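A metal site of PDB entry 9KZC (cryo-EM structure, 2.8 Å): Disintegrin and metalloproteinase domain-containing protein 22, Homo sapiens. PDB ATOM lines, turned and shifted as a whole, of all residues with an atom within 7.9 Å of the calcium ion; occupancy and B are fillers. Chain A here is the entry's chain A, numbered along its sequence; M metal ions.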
ATOM      1  N   TYR A   8     -19.050  20.396 -18.628  1.00  0.00           N
ATOM      2  CA  TYR A   8     -18.133  19.322 -18.965  1.00  0.00           C
ATOM      3  C   TYR A   8     -17.941  18.432 -17.753  1.00  0.00           C
ATOM      4  O   TYR A   8     -17.432  18.873 -16.728  1.00  0.00           O
ATOM      5  CB  TYR A   8     -16.775  19.880 -19.426  1.00  0.00           C
ATOM      6  CG  TYR A   8     -16.878  20.883 -20.556  1.00  0.00           C
ATOM      7  CD1 TYR A   8     -17.038  22.233 -20.297  1.00  0.00           C
ATOM      8  CD2 TYR A   8     -16.818  20.469 -21.880  1.00  0.00           C
ATOM      9  CE1 TYR A   8     -17.138  23.146 -21.332  1.00  0.00           C
ATOM     10  CE2 TYR A   8     -16.913  21.369 -22.918  1.00  0.00           C
ATOM     11  CZ  TYR A   8     -17.070  22.707 -22.637  1.00  0.00           C
ATOM     12  OH  TYR A   8     -17.166  23.614 -23.667  1.00  0.00           O
ATOM     13  N   ILE A   9     -18.367  17.175 -17.871  1.00  0.00           N
ATOM     14  CA  ILE A   9     -18.134  16.174 -16.837  1.00  0.00           C
ATOM     15  C   ILE A   9     -16.824  15.472 -17.154  1.00  0.00           C
ATOM     16  O   ILE A   9     -16.761  14.661 -18.092  1.00  0.00           O
ATOM     17  CB  ILE A   9     -19.294  15.179 -16.737  1.00  0.00           C
ATOM     18  CG1 ILE A   9     -20.613  15.899 -16.448  1.00  0.00           C
ATOM     19  CG2 ILE A   9     -19.000  14.130 -15.675  1.00  0.00           C
ATOM     20  CD1 ILE A   9     -21.834  15.075 -16.738  1.00  0.00           C
ATOM     21  N   GLU A  10     -15.779  15.776 -16.402  1.00  0.00           N
ATOM     22  CA  GLU A  10     -14.508  15.069 -16.514  1.00  0.00           C
ATOM     23  C   GLU A  10     -14.669  13.727 -15.804  1.00  0.00           C
ATOM     24  O   GLU A  10     -14.606  13.648 -14.584  1.00  0.00           O
ATOM     25  CB  GLU A  10     -13.370  15.879 -15.925  1.00  0.00           C
ATOM     26  CG  GLU A  10     -13.126  17.204 -16.630  1.00  0.00           C
ATOM     27  CD  GLU A  10     -12.026  18.016 -15.981  1.00  0.00           C
ATOM     28  OE1 GLU A  10     -11.618  17.664 -14.849  1.00  0.00           O
ATOM     29  OE2 GLU A  10     -11.560  18.997 -16.599  1.00  0.00           O
ATOM     30  N   LEU A  11     -14.880  12.674 -16.579  1.00  0.00           N
ATOM     31  CA  LEU A  11     -15.233  11.359 -16.051  1.00  0.00           C
ATOM     32  C   LEU A  11     -14.022  10.448 -16.045  1.00  0.00           C
ATOM     33  O   LEU A  11     -13.214  10.449 -16.985  1.00  0.00           O
ATOM     34  CB  LEU A  11     -16.360  10.744 -16.868  1.00  0.00           C
ATOM     35  CG  LEU A  11     -16.849   9.344 -16.471  1.00  0.00           C
ATOM     36  CD1 LEU A  11     -17.643   9.405 -15.185  1.00  0.00           C
ATOM     37  CD2 LEU A  11     -17.688   8.759 -17.590  1.00  0.00           C
ATOM     38  N   VAL A  56     -11.374  11.583 -18.952  1.00  0.00           N
ATOM     39  CA  VAL A  56     -10.060  12.160 -18.680  1.00  0.00           C
ATOM     40  C   VAL A  56      -9.097  11.160 -18.031  1.00  0.00           C
ATOM     41  O   VAL A  56      -7.884  11.421 -18.038  1.00  0.00           O
ATOM     42  CB  VAL A  56     -10.176  13.419 -17.802  1.00  0.00           C
ATOM     43  CG1 VAL A  56     -11.075  14.445 -18.468  1.00  0.00           C
ATOM     44  CG2 VAL A  56     -10.709  13.074 -16.415  1.00  0.00           C
ATOM     45  N   LYS A  91      -7.776  13.592 -10.588  1.00  0.00           N
ATOM     46  CA  LYS A  91      -8.757  14.674 -10.438  1.00  0.00           C
ATOM     47  C   LYS A  91      -9.824  14.531 -11.519  1.00  0.00           C
ATOM     48  O   LYS A  91      -9.518  14.594 -12.709  1.00  0.00           O
ATOM     49  CB  LYS A  91      -8.069  16.033 -10.526  1.00  0.00           C
ATOM     50  CG  LYS A  91      -6.992  16.267  -9.478  1.00  0.00           C
ATOM     51  CD  LYS A  91      -7.584  16.298  -8.082  1.00  0.00           C
ATOM     52  CE  LYS A  91      -6.544  16.711  -7.061  1.00  0.00           C
ATOM     53  NZ  LYS A  91      -5.471  15.690  -6.911  1.00  0.00           N
ATOM     54  N   SER A  92     -11.076  14.348 -11.092  1.00  0.00           N
ATOM     55  CA  SER A  92     -12.183  14.193 -12.013  1.00  0.00           C
ATOM     56  C   SER A  92     -13.467  14.641 -11.332  1.00  0.00           C
ATOM     57  O   SER A  92     -13.549  14.682 -10.099  1.00  0.00           O
ATOM     58  CB  SER A  92     -12.311  12.748 -12.503  1.00  0.00           C
ATOM     59  OG  SER A  92     -12.239  11.835 -11.419  1.00  0.00           O
ATOM     60  N   ASP A  93     -14.466  14.970 -12.156  1.00  0.00           N
ATOM     61  CA  ASP A  93     -15.762  15.345 -11.609  1.00  0.00           C
ATOM     62  C   ASP A  93     -16.501  14.137 -11.056  1.00  0.00           C
ATOM     63  O   ASP A  93     -17.141  14.216 -10.005  1.00  0.00           O
ATOM     64  CB  ASP A  93     -16.592  16.050 -12.681  1.00  0.00           C
ATOM     65  CG  ASP A  93     -15.885  17.237 -13.283  1.00  0.00           C
ATOM     66  OD1 ASP A  93     -14.854  17.654 -12.721  1.00  0.00           O
ATOM     67  OD2 ASP A  93     -16.349  17.764 -14.312  1.00  0.00           O
ATOM     68  N   ALA A  94     -16.438  13.008 -11.759  1.00  0.00           N
ATOM     69  CA  ALA A  94     -17.081  11.783 -11.328  1.00  0.00           C
ATOM     70  C   ALA A  94     -16.161  10.601 -11.593  1.00  0.00           C
ATOM     71  O   ALA A  94     -15.365  10.621 -12.536  1.00  0.00           O
ATOM     72  CB  ALA A  94     -18.432  11.564 -12.033  1.00  0.00           C
ATOM     73  N   CYS A 117     -18.939  16.301  -8.252  1.00  0.00           N
ATOM     74  CA  CYS A 117     -17.942  17.245  -7.749  1.00  0.00           C
ATOM     75  C   CYS A 117     -17.626  17.028  -6.282  1.00  0.00           C
ATOM     76  O   CYS A 117     -17.195  17.954  -5.588  1.00  0.00           O
ATOM     77  CB  CYS A 117     -18.373  18.698  -7.989  1.00  0.00           C
ATOM     78  SG  CYS A 117     -18.958  19.045  -9.659  1.00  0.00           S
ATOM     79  N   GLY A 199     -22.957  21.322  -8.959  1.00  0.00           N
ATOM     80  CA  GLY A 199     -22.167  21.106 -10.163  1.00  0.00           C
ATOM     81  C   GLY A 199     -21.294  22.278 -10.541  1.00  0.00           C
ATOM     82  O   GLY A 199     -21.149  22.591 -11.731  1.00  0.00           O
ATOM     83  N   ALA A 200     -20.692  22.944  -9.548  1.00  0.00           N
ATOM     84  CA  ALA A 200     -19.818  24.078  -9.820  1.00  0.00           C
ATOM     85  C   ALA A 200     -18.505  23.667 -10.466  1.00  0.00           C
ATOM     86  O   ALA A 200     -17.772  24.540 -10.948  1.00  0.00           O
ATOM     87  CB  ALA A 200     -19.549  24.853  -8.534  1.00  0.00           C
ATOM     88  N   CYS A 201     -18.193  22.380 -10.488  1.00  0.00           N
ATOM     89  CA  CYS A 201     -16.951  21.883 -11.069  1.00  0.00           C
ATOM     90  C   CYS A 201     -17.088  21.543 -12.550  1.00  0.00           C
ATOM     91  O   CYS A 201     -16.106  21.122 -13.165  1.00  0.00           O
ATOM     92  CB  CYS A 201     -16.464  20.650 -10.300  1.00  0.00           C
ATOM     93  SG  CYS A 201     -17.269  19.108 -10.784  1.00  0.00           S
ATOM     94  N   LEU A 202     -18.277  21.708 -13.129  1.00  0.00           N
ATOM     95  CA  LEU A 202     -18.544  21.326 -14.506  1.00  0.00           C
ATOM     96  C   LEU A 202     -18.324  22.476 -15.494  1.00  0.00           C
ATOM     97  O   LEU A 202     -18.654  22.325 -16.675  1.00  0.00           O
ATOM     98  CB  LEU A 202     -19.971  20.805 -14.648  1.00  0.00           C
ATOM     99  CG  LEU A 202     -20.419  19.704 -13.683  1.00  0.00           C
ATOM    100  CD1 LEU A 202     -21.905  19.448 -13.820  1.00  0.00           C
ATOM    101  CD2 LEU A 202     -19.623  18.435 -13.924  1.00  0.00           C
ATOM    102  N   PHE A 203     -17.793  23.601 -15.040  1.00  0.00           N
ATOM    103  CA  PHE A 203     -17.665  24.786 -15.870  1.00  0.00           C
ATOM    104  C   PHE A 203     -16.243  25.024 -16.370  1.00  0.00           C
ATOM    105  O   PHE A 203     -15.964  26.080 -16.928  1.00  0.00           O
ATOM    106  CB  PHE A 203     -18.170  26.014 -15.114  1.00  0.00           C
ATOM    107  CG  PHE A 203     -19.637  25.962 -14.812  1.00  0.00           C
ATOM    108  CD1 PHE A 203     -20.563  26.387 -15.747  1.00  0.00           C
ATOM    109  CD2 PHE A 203     -20.087  25.453 -13.598  1.00  0.00           C
ATOM    110  CE1 PHE A 203     -21.913  26.323 -15.469  1.00  0.00           C
ATOM    111  CE2 PHE A 203     -21.442  25.390 -13.334  1.00  0.00           C
ATOM    112  CZ  PHE A 203     -22.346  25.824 -14.261  1.00  0.00           C
ATOM    113  N   ASN A 204     -15.349  24.053 -16.180  1.00  0.00           N
ATOM    114  CA  ASN A 204     -14.018  24.115 -16.762  1.00  0.00           C
ATOM    115  C   ASN A 204     -13.931  23.187 -17.963  1.00  0.00           C
ATOM    116  O   ASN A 204     -14.423  22.050 -17.924  1.00  0.00           O
ATOM    117  CB  ASN A 204     -12.936  23.776 -15.735  1.00  0.00           C
ATOM    118  CG  ASN A 204     -13.156  22.417 -15.078  1.00  0.00           C
ATOM    119  OD1 ASN A 204     -14.164  21.752 -15.304  1.00  0.00           O
ATOM    120  ND2 ASN A 204     -12.188  22.005 -14.266  1.00  0.00           N
ATOM    121  N   LYS A 205     -13.327  23.667 -19.033  1.00  0.00           N
ATOM    122  CA  LYS A 205     -13.171  22.841 -20.222  1.00  0.00           C
ATOM    123  C   LYS A 205     -11.898  22.019 -20.116  1.00  0.00           C
ATOM    124  O   LYS A 205     -10.822  22.576 -19.865  1.00  0.00           O
ATOM    125  CB  LYS A 205     -13.122  23.703 -21.476  1.00  0.00           C
ATOM    126  CG  LYS A 205     -13.233  22.916 -22.771  1.00  0.00           C
ATOM    127  CD  LYS A 205     -13.050  23.807 -23.979  1.00  0.00           C
ATOM    128  CE  LYS A 205     -14.063  23.481 -25.055  1.00  0.00           C
ATOM    129  NZ  LYS A 205     -14.323  24.649 -25.953  1.00  0.00           N
ATOM    130  N   PRO A 206     -11.967  20.699 -20.270  1.00  0.00           N
ATOM    131  CA  PRO A 206     -10.770  19.860 -20.104  1.00  0.00           C
ATOM    132  C   PRO A 206      -9.681  20.227 -21.101  1.00  0.00           C
ATOM    133  O   PRO A 206      -9.958  20.542 -22.262  1.00  0.00           O
ATOM    134  CB  PRO A 206     -11.295  18.438 -20.339  1.00  0.00           C
ATOM    135  CG  PRO A 206     -12.771  18.530 -20.137  1.00  0.00           C
ATOM    136  CD  PRO A 206     -13.166  19.900 -20.591  1.00  0.00           C
HETATM  137 CA    CA M   1     -14.252  19.724 -13.877  1.00  0.00          CA
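SG of Cys 117 forms a disulfide with SG of Cys 201 (2.0 Å). O of Glu 10 is in hydrogen-bond range of N of Asp 93 (2.8 Å). N of Cys 117 sits at hydrogen-bond distance from O of Asp 93, at 3.3 Å. O of Glu 10 lies within hydrogen-bond range of N of Ala 94 (3.4 Å).
OE1 of Glu 10 touches the calcium ion, 3.5 Å away. Of the 18 residues printed, 4 come within 4 Å of the calcium ion.
The backbone carbonyl oxygen (O) of Cys 201 binds the calcium ion (2.4 Å). OD1 of Asp 93 is bound to the calcium ion (2.4 Å). The side-chain amide oxygen (OD1) of Asn 204 binds the calcium ion, 2.5 Å away. The calcium ion has three donor atoms within binding distance. Slightly farther from the calcium ion lies the side-chain carboxylate (OD2) of Asp 93 (2.9 Å). Slightly farther from the calcium ion lies ND2 of Asn 204 (3.1 Å).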
